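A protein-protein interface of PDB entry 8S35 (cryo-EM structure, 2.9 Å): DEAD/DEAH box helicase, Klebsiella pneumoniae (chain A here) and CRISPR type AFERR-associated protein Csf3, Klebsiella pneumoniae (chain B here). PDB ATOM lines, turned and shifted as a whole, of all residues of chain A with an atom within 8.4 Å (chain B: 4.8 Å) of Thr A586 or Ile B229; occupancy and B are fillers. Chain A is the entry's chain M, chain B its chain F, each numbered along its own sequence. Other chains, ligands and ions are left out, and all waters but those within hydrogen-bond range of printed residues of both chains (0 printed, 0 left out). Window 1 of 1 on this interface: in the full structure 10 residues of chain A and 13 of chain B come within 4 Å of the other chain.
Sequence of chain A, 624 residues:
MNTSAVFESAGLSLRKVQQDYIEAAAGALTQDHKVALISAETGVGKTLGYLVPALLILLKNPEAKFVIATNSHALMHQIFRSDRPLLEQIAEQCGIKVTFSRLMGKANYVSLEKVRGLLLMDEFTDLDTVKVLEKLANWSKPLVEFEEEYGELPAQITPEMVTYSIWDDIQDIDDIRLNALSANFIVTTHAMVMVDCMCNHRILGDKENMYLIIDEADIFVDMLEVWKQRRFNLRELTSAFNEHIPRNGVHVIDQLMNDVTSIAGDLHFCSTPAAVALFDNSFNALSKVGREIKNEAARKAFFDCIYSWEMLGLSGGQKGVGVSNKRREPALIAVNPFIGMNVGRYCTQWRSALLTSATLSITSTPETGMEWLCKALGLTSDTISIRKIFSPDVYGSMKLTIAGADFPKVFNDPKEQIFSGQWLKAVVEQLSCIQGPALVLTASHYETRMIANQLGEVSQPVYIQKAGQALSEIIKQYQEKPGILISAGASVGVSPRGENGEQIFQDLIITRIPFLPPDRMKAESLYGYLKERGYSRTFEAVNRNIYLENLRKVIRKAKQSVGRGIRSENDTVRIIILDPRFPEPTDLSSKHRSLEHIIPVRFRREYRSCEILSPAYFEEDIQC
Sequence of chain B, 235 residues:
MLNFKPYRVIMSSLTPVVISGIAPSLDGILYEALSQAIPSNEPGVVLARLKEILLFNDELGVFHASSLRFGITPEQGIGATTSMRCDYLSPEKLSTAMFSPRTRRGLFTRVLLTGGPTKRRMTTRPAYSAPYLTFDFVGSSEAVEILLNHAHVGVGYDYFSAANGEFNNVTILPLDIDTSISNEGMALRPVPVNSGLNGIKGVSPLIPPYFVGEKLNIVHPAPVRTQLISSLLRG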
ATOM      1  N   ILE A 402      -2.218 -10.564   9.985  1.00  0.00           N
ATOM      2  CA  ILE A 402      -0.847 -10.300  10.405  1.00  0.00           C
ATOM      3  C   ILE A 402      -0.662  -8.832  10.741  1.00  0.00           C
ATOM      4  O   ILE A 402      -1.334  -7.950  10.196  1.00  0.00           O
ATOM      5  CB  ILE A 402       0.195 -10.692   9.332  1.00  0.00           C
ATOM      6  CG1 ILE A 402      -0.114 -10.033   7.979  1.00  0.00           C
ATOM      7  CG2 ILE A 402       0.249 -12.166   9.174  1.00  0.00           C
ATOM      8  CD1 ILE A 402       1.107  -9.874   7.099  1.00  0.00           C
ATOM      9  N   PRO A 583       7.104 -11.787   8.710  1.00  0.00           N
ATOM     10  CA  PRO A 583       7.305 -11.258   7.357  1.00  0.00           C
ATOM     11  C   PRO A 583       5.987 -11.081   6.620  1.00  0.00           C
ATOM     12  O   PRO A 583       5.153 -11.988   6.580  1.00  0.00           O
ATOM     13  CB  PRO A 583       8.184 -12.319   6.691  1.00  0.00           C
ATOM     14  CG  PRO A 583       7.842 -13.566   7.393  1.00  0.00           C
ATOM     15  CD  PRO A 583       7.599 -13.172   8.819  1.00  0.00           C
ATOM     16  N   GLU A 584       5.808  -9.903   6.036  1.00  0.00           N
ATOM     17  CA  GLU A 584       4.654  -9.659   5.193  1.00  0.00           C
ATOM     18  C   GLU A 584       4.777 -10.479   3.909  1.00  0.00           C
ATOM     19  O   GLU A 584       5.887 -10.785   3.468  1.00  0.00           O
ATOM     20  CB  GLU A 584       4.532  -8.176   4.855  1.00  0.00           C
ATOM     21  CG  GLU A 584       3.777  -7.365   5.898  1.00  0.00           C
ATOM     22  CD  GLU A 584       3.530  -5.932   5.463  1.00  0.00           C
ATOM     23  OE1 GLU A 584       3.334  -5.700   4.252  1.00  0.00           O
ATOM     24  OE2 GLU A 584       3.532  -5.037   6.334  1.00  0.00           O
ATOM     25  N   PRO A 585       3.653 -10.864   3.294  1.00  0.00           N
ATOM     26  CA  PRO A 585       3.759 -11.657   2.057  1.00  0.00           C
ATOM     27  C   PRO A 585       4.495 -10.925   0.952  1.00  0.00           C
ATOM     28  O   PRO A 585       5.276 -11.543   0.217  1.00  0.00           O
ATOM     29  CB  PRO A 585       2.297 -11.930   1.678  1.00  0.00           C
ATOM     30  CG  PRO A 585       1.486 -11.571   2.865  1.00  0.00           C
ATOM     31  CD  PRO A 585       2.253 -10.553   3.627  1.00  0.00           C
ATOM     32  N   THR A 586       4.280  -9.617   0.823  1.00  0.00           N
ATOM     33  CA  THR A 586       4.950  -8.843  -0.212  1.00  0.00           C
ATOM     34  C   THR A 586       6.403  -8.545   0.130  1.00  0.00           C
ATOM     35  O   THR A 586       7.190  -8.253  -0.778  1.00  0.00           O
ATOM     36  CB  THR A 586       4.206  -7.528  -0.452  1.00  0.00           C
ATOM     37  OG1 THR A 586       4.295  -6.704   0.717  1.00  0.00           O
ATOM     38  CG2 THR A 586       2.743  -7.792  -0.772  1.00  0.00           C
ATOM     39  N   ASP A 587       6.776  -8.611   1.408  1.00  0.00           N
ATOM     40  CA  ASP A 587       8.152  -8.353   1.836  1.00  0.00           C
ATOM     41  C   ASP A 587       8.898  -9.683   1.882  1.00  0.00           C
ATOM     42  O   ASP A 587       9.145 -10.266   2.938  1.00  0.00           O
ATOM     43  CB  ASP A 587       8.170  -7.647   3.185  1.00  0.00           C
ATOM     44  CG  ASP A 587       9.531  -7.070   3.525  1.00  0.00           C
ATOM     45  OD1 ASP A 587      10.531  -7.477   2.896  1.00  0.00           O
ATOM     46  OD2 ASP A 587       9.602  -6.208   4.425  1.00  0.00           O
ATOM     47  N   LEU A 588       9.274 -10.162   0.695  1.00  0.00           N
ATOM     48  CA  LEU A 588       9.994 -11.426   0.587  1.00  0.00           C
ATOM     49  C   LEU A 588      11.439 -11.325   1.059  1.00  0.00           C
ATOM     50  O   LEU A 588      12.090 -12.364   1.212  1.00  0.00           O
ATOM     51  CB  LEU A 588       9.961 -11.925  -0.860  1.00  0.00           C
ATOM     52  CG  LEU A 588       8.754 -12.753  -1.313  1.00  0.00           C
ATOM     53  CD1 LEU A 588       8.885 -13.100  -2.786  1.00  0.00           C
ATOM     54  CD2 LEU A 588       8.598 -14.024  -0.494  1.00  0.00           C
ATOM     55  N   SER A 589      11.950 -10.115   1.294  1.00  0.00           N
ATOM     56  CA  SER A 589      13.326  -9.902   1.722  1.00  0.00           C
ATOM     57  C   SER A 589      13.431  -9.595   3.212  1.00  0.00           C
ATOM     58  O   SER A 589      14.480  -9.129   3.670  1.00  0.00           O
ATOM     59  CB  SER A 589      13.957  -8.773   0.906  1.00  0.00           C
ATOM     60  OG  SER A 589      13.038  -7.711   0.721  1.00  0.00           O
ATOM     61  N   SER A 590      12.373  -9.851   3.978  1.00  0.00           N
ATOM     62  CA  SER A 590      12.430  -9.622   5.414  1.00  0.00           C
ATOM     63  C   SER A 590      13.478 -10.529   6.046  1.00  0.00           C
ATOM     64  O   SER A 590      13.742 -11.636   5.569  1.00  0.00           O
ATOM     65  CB  SER A 590      11.065  -9.877   6.051  1.00  0.00           C
ATOM     66  OG  SER A 590      11.194 -10.124   7.440  1.00  0.00           O
ATOM     67  N   ARG A 593      12.413 -14.107   7.049  1.00  0.00           N
ATOM     68  CA  ARG A 593      11.580 -14.671   5.994  1.00  0.00           C
ATOM     69  C   ARG A 593      11.244 -16.127   6.286  1.00  0.00           C
ATOM     70  O   ARG A 593      10.149 -16.590   5.947  1.00  0.00           O
ATOM     71  CB  ARG A 593      12.291 -14.513   4.644  1.00  0.00           C
ATOM     72  CG  ARG A 593      11.845 -15.437   3.501  1.00  0.00           C
ATOM     73  CD  ARG A 593      10.360 -15.340   3.139  1.00  0.00           C
ATOM     74  NE  ARG A 593       9.794 -14.003   3.272  1.00  0.00           N
ATOM     75  CZ  ARG A 593       8.507 -13.719   3.109  1.00  0.00           C
ATOM     76  NH1 ARG A 593       7.618 -14.660   2.828  1.00  0.00           N
ATOM     77  NH2 ARG A 593       8.100 -12.459   3.224  1.00  0.00           N
ATOM     78  N   TYR A 607      -1.691 -17.484   3.155  1.00  0.00           N
ATOM     79  CA  TYR A 607      -0.662 -16.582   3.655  1.00  0.00           C
ATOM     80  C   TYR A 607      -0.482 -15.402   2.710  1.00  0.00           C
ATOM     81  O   TYR A 607      -0.319 -14.261   3.156  1.00  0.00           O
ATOM     82  CB  TYR A 607       0.664 -17.321   3.854  1.00  0.00           C
ATOM     83  CG  TYR A 607       1.854 -16.398   3.999  1.00  0.00           C
ATOM     84  CD1 TYR A 607       1.888 -15.428   4.989  1.00  0.00           C
ATOM     85  CD2 TYR A 607       2.939 -16.489   3.139  1.00  0.00           C
ATOM     86  CE1 TYR A 607       2.966 -14.582   5.127  1.00  0.00           C
ATOM     87  CE2 TYR A 607       4.025 -15.644   3.269  1.00  0.00           C
ATOM     88  CZ  TYR A 607       4.031 -14.692   4.265  1.00  0.00           C
ATOM     89  OH  TYR A 607       5.104 -13.843   4.405  1.00  0.00           O
ATOM     90  N   ARG A 608      -0.508 -15.657   1.400  1.00  0.00           N
ATOM     91  CA  ARG A 608      -0.331 -14.576   0.440  1.00  0.00           C
ATOM     92  C   ARG A 608      -1.477 -13.575   0.507  1.00  0.00           C
ATOM     93  O   ARG A 608      -1.251 -12.362   0.440  1.00  0.00           O
ATOM     94  CB  ARG A 608      -0.202 -15.150  -0.969  1.00  0.00           C
ATOM     95  CG  ARG A 608       1.175 -15.709  -1.270  1.00  0.00           C
ATOM     96  CD  ARG A 608       1.212 -16.388  -2.622  1.00  0.00           C
ATOM     97  NE  ARG A 608       0.829 -17.792  -2.535  1.00  0.00           N
ATOM     98  CZ  ARG A 608       1.625 -18.768  -2.119  1.00  0.00           C
ATOM     99  NH1 ARG A 608       2.872 -18.536  -1.741  1.00  0.00           N
ATOM    100  NH2 ARG A 608       1.157 -20.013  -2.080  1.00  0.00           N
ATOM    101  N   SER A 609      -2.709 -14.060   0.647  1.00  0.00           N
ATOM    102  CA  SER A 609      -3.898 -13.209   0.711  1.00  0.00           C
ATOM    103  C   SER A 609      -4.331 -13.134   2.171  1.00  0.00           C
ATOM    104  O   SER A 609      -5.166 -13.915   2.631  1.00  0.00           O
ATOM    105  CB  SER A 609      -5.005 -13.757  -0.181  1.00  0.00           C
ATOM    106  OG  SER A 609      -5.425 -15.036   0.261  1.00  0.00           O
ATOM    107  N   CYS A 610      -3.753 -12.184   2.904  1.00  0.00           N
ATOM    108  CA  CYS A 610      -4.005 -12.024   4.328  1.00  0.00           C
ATOM    109  C   CYS A 610      -4.273 -10.566   4.666  1.00  0.00           C
ATOM    110  O   CYS A 610      -3.661  -9.662   4.090  1.00  0.00           O
ATOM    111  CB  CYS A 610      -2.816 -12.530   5.144  1.00  0.00           C
ATOM    112  SG  CYS A 610      -1.294 -11.603   4.859  1.00  0.00           S
ATOM    113  N   ILE A 612      -3.671  -7.438   6.492  1.00  0.00           N
ATOM    114  CA  ILE A 612      -2.557  -6.837   7.216  1.00  0.00           C
ATOM    115  C   ILE A 612      -3.112  -5.732   8.104  1.00  0.00           C
ATOM    116  O   ILE A 612      -3.780  -4.812   7.620  1.00  0.00           O
ATOM    117  CB  ILE A 612      -1.484  -6.295   6.258  1.00  0.00           C
ATOM    118  CG1 ILE A 612      -1.177  -7.326   5.161  1.00  0.00           C
ATOM    119  CG2 ILE A 612      -0.221  -5.935   7.049  1.00  0.00           C
ATOM    120  CD1 ILE A 612      -0.109  -6.907   4.165  1.00  0.00           C
ATOM    121  N   PRO A 615      -0.080  -2.551   7.291  1.00  0.00           N
ATOM    122  CA  PRO A 615       0.889  -2.725   6.206  1.00  0.00           C
ATOM    123  C   PRO A 615       1.712  -1.468   5.985  1.00  0.00           C
ATOM    124  O   PRO A 615       1.235  -0.345   6.161  1.00  0.00           O
ATOM    125  CB  PRO A 615       0.009  -3.038   4.990  1.00  0.00           C
ATOM    126  CG  PRO A 615      -1.315  -2.444   5.318  1.00  0.00           C
ATOM    127  CD  PRO A 615      -1.468  -2.566   6.803  1.00  0.00           C
ATOM    128  N   ALA A 616       2.963  -1.673   5.590  1.00  0.00           N
ATOM    129  CA  ALA A 616       3.868  -0.587   5.251  1.00  0.00           C
ATOM    130  C   ALA A 616       3.915  -0.415   3.741  1.00  0.00           C
ATOM    131  O   ALA A 616       3.729  -1.371   2.984  1.00  0.00           O
ATOM    132  CB  ALA A 616       5.272  -0.858   5.789  1.00  0.00           C
ATOM    133  N   TYR A 617       4.170   0.819   3.306  1.00  0.00           N
ATOM    134  CA  TYR A 617       4.274   1.121   1.879  1.00  0.00           C
ATOM    135  C   TYR A 617       2.958   0.798   1.177  1.00  0.00           C
ATOM    136  O   TYR A 617       2.933   0.289   0.055  1.00  0.00           O
ATOM    137  CB  TYR A 617       5.446   0.367   1.241  1.00  0.00           C
ATOM    138  CG  TYR A 617       6.675   0.262   2.127  1.00  0.00           C
ATOM    139  CD1 TYR A 617       7.429  -0.902   2.163  1.00  0.00           C
ATOM    140  CD2 TYR A 617       7.110   1.343   2.887  1.00  0.00           C
ATOM    141  CE1 TYR A 617       8.550  -1.002   2.965  1.00  0.00           C
ATOM    142  CE2 TYR A 617       8.231   1.251   3.689  1.00  0.00           C
ATOM    143  CZ  TYR A 617       8.950   0.078   3.719  1.00  0.00           C
ATOM    144  OH  TYR A 617      10.071  -0.020   4.511  1.00  0.00           O
ATOM    145  N   PHE A 618       1.852   1.102   1.857  1.00  0.00           N
ATOM    146  CA  PHE A 618       0.510   0.739   1.405  1.00  0.00           C
ATOM    147  C   PHE A 618      -0.018   1.794   0.432  1.00  0.00           C
ATOM    148  O   PHE A 618      -0.988   2.509   0.692  1.00  0.00           O
ATOM    149  CB  PHE A 618      -0.415   0.570   2.601  1.00  0.00           C
ATOM    150  CG  PHE A 618      -1.705  -0.124   2.275  1.00  0.00           C
ATOM    151  CD1 PHE A 618      -1.722  -1.474   1.967  1.00  0.00           C
ATOM    152  CD2 PHE A 618      -2.901   0.573   2.276  1.00  0.00           C
ATOM    153  CE1 PHE A 618      -2.907  -2.115   1.667  1.00  0.00           C
ATOM    154  CE2 PHE A 618      -4.089  -0.063   1.978  1.00  0.00           C
ATOM    155  CZ  PHE A 618      -4.093  -1.409   1.672  1.00  0.00           C
ATOM    156  N   GLN A 623       5.946   3.450 -10.931  1.00  0.00           N
ATOM    157  CA  GLN A 623       7.010   2.775 -11.670  1.00  0.00           C
ATOM    158  C   GLN A 623       6.783   1.262 -11.650  1.00  0.00           C
ATOM    159  O   GLN A 623       7.574   0.483 -11.121  1.00  0.00           O
ATOM    160  CB  GLN A 623       8.366   3.137 -11.084  1.00  0.00           C
ATOM    161  CG  GLN A 623       9.545   2.643 -11.921  1.00  0.00           C
ATOM    162  CD  GLN A 623      10.536   1.780 -11.150  1.00  0.00           C
ATOM    163  OE1 GLN A 623      10.266   1.325 -10.038  1.00  0.00           O
ATOM    164  NE2 GLN A 623      11.698   1.552 -11.748  1.00  0.00           N
ATOM    165  N   CYS A 624       5.667   0.856 -12.246  1.00  0.00           N
ATOM    166  CA  CYS A 624       5.289  -0.549 -12.305  1.00  0.00           C
ATOM    167  C   CYS A 624       5.962  -1.230 -13.491  1.00  0.00           C
ATOM    168  O   CYS A 624       5.322  -1.948 -14.259  1.00  0.00           O
ATOM    169  CB  CYS A 624       3.766  -0.687 -12.399  1.00  0.00           C
ATOM    170  SG  CYS A 624       2.858   0.626 -11.554  1.00  0.00           S
ATOM    171  N   ILE B  72       9.842  -5.870  -8.723  1.00  0.00           N
ATOM    172  CA  ILE B  72      10.391  -4.706  -8.038  1.00  0.00           C
ATOM    173  C   ILE B  72       9.484  -4.376  -6.865  1.00  0.00           C
ATOM    174  O   ILE B  72       8.258  -4.332  -7.011  1.00  0.00           O
ATOM    175  CB  ILE B  72      10.532  -3.498  -8.982  1.00  0.00           C
ATOM    176  CG1 ILE B  72       9.280  -3.324  -9.846  1.00  0.00           C
ATOM    177  CG2 ILE B  72      11.755  -3.667  -9.862  1.00  0.00           C
ATOM    178  CD1 ILE B  72       9.126  -1.940 -10.423  1.00  0.00           C
ATOM    179  N   THR B  73      10.082  -4.153  -5.712  1.00  0.00           N
ATOM    180  CA  THR B  73       9.376  -3.781  -4.500  1.00  0.00           C
ATOM    181  C   THR B  73       9.462  -2.280  -4.296  1.00  0.00           C
ATOM    182  O   THR B  73      10.280  -1.601  -4.920  1.00  0.00           O
ATOM    183  CB  THR B  73       9.977  -4.515  -3.301  1.00  0.00           C
ATOM    184  OG1 THR B  73      11.128  -3.800  -2.833  1.00  0.00           O
ATOM    185  CG2 THR B  73      10.382  -5.925  -3.681  1.00  0.00           C
ATOM    186  N   PRO B  74       8.630  -1.710  -3.420  1.00  0.00           N
ATOM    187  CA  PRO B  74       8.760  -0.273  -3.132  1.00  0.00           C
ATOM    188  C   PRO B  74      10.088   0.109  -2.499  1.00  0.00           C
ATOM    189  O   PRO B  74      10.380   1.308  -2.413  1.00  0.00           O
ATOM    190  CB  PRO B  74       7.588   0.012  -2.182  1.00  0.00           C
ATOM    191  CG  PRO B  74       7.141  -1.313  -1.687  1.00  0.00           C
ATOM    192  CD  PRO B  74       7.440  -2.286  -2.774  1.00  0.00           C
ATOM    193  N   TYR B 132      13.877  -8.793  -7.297  1.00  0.00           N
ATOM    194  CA  TYR B 132      13.357 -10.132  -7.535  1.00  0.00           C
ATOM    195  C   TYR B 132      13.231 -10.391  -9.026  1.00  0.00           C
ATOM    196  O   TYR B 132      13.099  -9.470  -9.831  1.00  0.00           O
ATOM    197  CB  TYR B 132      11.994 -10.333  -6.863  1.00  0.00           C
ATOM    198  CG  TYR B 132      12.048 -10.197  -5.367  1.00  0.00           C
ATOM    199  CD1 TYR B 132      11.908  -8.961  -4.763  1.00  0.00           C
ATOM    200  CD2 TYR B 132      12.253 -11.302  -4.559  1.00  0.00           C
ATOM    201  CE1 TYR B 132      11.969  -8.828  -3.401  1.00  0.00           C
ATOM    202  CE2 TYR B 132      12.311 -11.177  -3.191  1.00  0.00           C
ATOM    203  CZ  TYR B 132      12.171  -9.935  -2.620  1.00  0.00           C
ATOM    204  OH  TYR B 132      12.223  -9.793  -1.257  1.00  0.00           O
ATOM    205  N   GLN B 227       7.329  -5.503 -12.678  1.00  0.00           N
ATOM    206  CA  GLN B 227       6.030  -5.578 -12.031  1.00  0.00           C
ATOM    207  C   GLN B 227       6.220  -5.483 -10.528  1.00  0.00           C
ATOM    208  O   GLN B 227       7.236  -5.924  -9.987  1.00  0.00           O
ATOM    209  CB  GLN B 227       5.300  -6.878 -12.383  1.00  0.00           C
ATOM    210  CG  GLN B 227       3.790  -6.752 -12.370  1.00  0.00           C
ATOM    211  CD  GLN B 227       3.260  -6.020 -13.584  1.00  0.00           C
ATOM    212  OE1 GLN B 227       4.008  -5.350 -14.294  1.00  0.00           O
ATOM    213  NE2 GLN B 227       1.961  -6.144 -13.829  1.00  0.00           N
ATOM    214  N   LEU B 228       5.229  -4.907  -9.856  1.00  0.00           N
ATOM    215  CA  LEU B 228       5.280  -4.821  -8.406  1.00  0.00           C
ATOM    216  C   LEU B 228       5.225  -6.217  -7.804  1.00  0.00           C
ATOM    217  O   LEU B 228       4.471  -7.078  -8.263  1.00  0.00           O
ATOM    218  CB  LEU B 228       4.127  -3.969  -7.879  1.00  0.00           C
ATOM    219  CG  LEU B 228       4.381  -2.461  -7.860  1.00  0.00           C
ATOM    220  CD1 LEU B 228       3.078  -1.706  -7.662  1.00  0.00           C
ATOM    221  CD2 LEU B 228       5.383  -2.089  -6.776  1.00  0.00           C
ATOM    222  N   ILE B 229       6.035  -6.441  -6.769  1.00  0.00           N
ATOM    223  CA  ILE B 229       6.066  -7.757  -6.142  1.00  0.00           C
ATOM    224  C   ILE B 229       4.712  -8.087  -5.532  1.00  0.00           C
ATOM    225  O   ILE B 229       4.278  -9.245  -5.534  1.00  0.00           O
ATOM    226  CB  ILE B 229       7.193  -7.828  -5.095  1.00  0.00           C
ATOM    227  CG1 ILE B 229       7.361  -9.264  -4.596  1.00  0.00           C
ATOM    228  CG2 ILE B 229       6.914  -6.890  -3.921  1.00  0.00           C
ATOM    229  CD1 ILE B 229       8.709  -9.534  -3.981  1.00  0.00           C
ATOM    230  N   SER B 230       4.023  -7.077  -4.995  1.00  0.00           N
ATOM    231  CA  SER B 230       2.690  -7.308  -4.453  1.00  0.00           C
ATOM    232  C   SER B 230       1.741  -7.798  -5.537  1.00  0.00           C
ATOM    233  O   SER B 230       0.958  -8.729  -5.313  1.00  0.00           O
ATOM    234  CB  SER B 230       2.156  -6.028  -3.815  1.00  0.00           C
ATOM    235  OG  SER B 230       2.009  -5.005  -4.783  1.00  0.00           O
ATOM    236  N   SER B 231       1.800  -7.187  -6.721  1.00  0.00           N
ATOM    237  CA  SER B 231       0.953  -7.637  -7.818  1.00  0.00           C
ATOM    238  C   SER B 231       1.350  -9.025  -8.297  1.00  0.00           C
ATOM    239  O   SER B 231       0.487  -9.803  -8.717  1.00  0.00           O
ATOM    240  CB  SER B 231       1.023  -6.640  -8.972  1.00  0.00           C
ATOM    241  OG  SER B 231       2.368  -6.328  -9.289  1.00  0.00           O
ATOM    242  N   LEU B 232       2.641  -9.357  -8.240  1.00  0.00           N
ATOM    243  CA  LEU B 232       3.073 -10.675  -8.687  1.00  0.00           C
ATOM    244  C   LEU B 232       2.629 -11.766  -7.726  1.00  0.00           C
ATOM    245  O   LEU B 232       2.331 -12.886  -8.156  1.00  0.00           O
ATOM    246  CB  LEU B 232       4.591 -10.703  -8.848  1.00  0.00           C
ATOM    247  CG  LEU B 232       5.151  -9.857  -9.991  1.00  0.00           C
ATOM    248  CD1 LEU B 232       6.641  -9.644  -9.805  1.00  0.00           C
ATOM    249  CD2 LEU B 232       4.863 -10.501 -11.339  1.00  0.00           C
ATOM    250  N   LEU B 233       2.571 -11.464  -6.430  1.00  0.00           N
ATOM    251  CA  LEU B 233       2.123 -12.438  -5.445  1.00  0.00           C
ATOM    252  C   LEU B 233       0.607 -12.540  -5.363  1.00  0.00           C
ATOM    253  O   LEU B 233       0.101 -13.422  -4.662  1.00  0.00           O
ATOM    254  CB  LEU B 233       2.682 -12.083  -4.068  1.00  0.00           C
ATOM    255  CG  LEU B 233       4.169 -12.382  -3.884  1.00  0.00           C
ATOM    256  CD1 LEU B 233       4.746 -11.509  -2.792  1.00  0.00           C
ATOM    257  CD2 LEU B 233       4.386 -13.852  -3.570  1.00  0.00           C
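The side-chain hydroxyl (OH) of Tyr B132 sits at hydrogen-bond distance from the backbone NH (N) of Ser A589, at 2.6 Å.
The backbone NH of Ile B72 lies within hydrogen-bond range of the backbone carbonyl oxygen of Gln B227, 2.9 Å away. N of Ile B229 is in hydrogen-bond range of O of Ile B72, at 3.1 Å. The side-chain carboxylate (OD1) of Asp A587 sits at hydrogen-bond distance from the side-chain hydroxyl (OG) of Ser A589 (3.3 Å). The backbone carbonyl oxygen (O) of Leu A588 is in hydrogen-bond range of the guanidinium group (NE) of Arg A593, at 3.5 Å.
Of the 11 printed residues of chain B, 7 touch a printed residue of chain A. Printed residues of chain B that touch a printed residue of chain A: Ile B72, Pro B74, Tyr B132, Gln B227, Ile B229, Ser B230 and Leu B233. Hydrophobic or aromatic side chains of chain B within 4 Å of the printed part of chain A: Ile B72, Pro B74, Tyr B132, Ile B229 and Leu B233. Of the 21 printed residues of chain A, 8 touch a printed residue of chain B. Printed residues of chain A that touch a printed residue of chain B: Pro A585, Thr A586, Leu A588, Ser A589, Arg A608, Tyr A617, Gln A623 and Cys A624. Hydrophobic or aromatic side chains of chain A that line the printed part of chain B: Leu A588 and Tyr A617. Among the printed residues, no Asp or Glu carboxylate lies within 4 Å of a Lys or Arg side-chain nitrogen of the other chain.
Thr A586 touches just these residues of chain B: Ile B229, Ser B230 and Leu B233. Of chain A, only Thr A586 and Leu A588 come within 4 Å of Ile B229. Ser B230 touches just one residue of chain A: Thr A586 (3.6 Å). Of the printed residues of chain B, Pro A585 touches Leu B233. Printed residues of chain B within 4 Å of Cys A624: Gln B227. Pro A583 touches none of the printed residues of chain B. Asp A587 touches none of the printed residues of chain B. The nearest residue of chain A that does not touch Ile B229 is Asp A587 (5.6 Å). The nearest printed residue of chain B that does not touch Leu A588 is Leu B233 (4.4 Å).
O of Pro A585 touches CD1 of Leu B233, 3.1 Å away. O of Thr A586 touches CG2 of Ile B229, 3.4 Å away. Ser B230 touches Thr A586 (CB to CG2, 3.6 Å). CD1 of Leu B233 touches CA of Thr A586, 3.7 Å away. Tyr B132 touches Leu A588. Leu A588 touches Ile B229 (CD1 to CD1, 3.8 Å). CD of Arg A608 touches O of Leu B233 (3.8 Å). Tyr A617 touches Pro B74 (CB to CG, 3.8 Å). O of Gln A623 touches CD1 of Ile B72 (3.0 Å). Gln B227 touches Cys A624 (OE1 to O, 3.6 Å).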
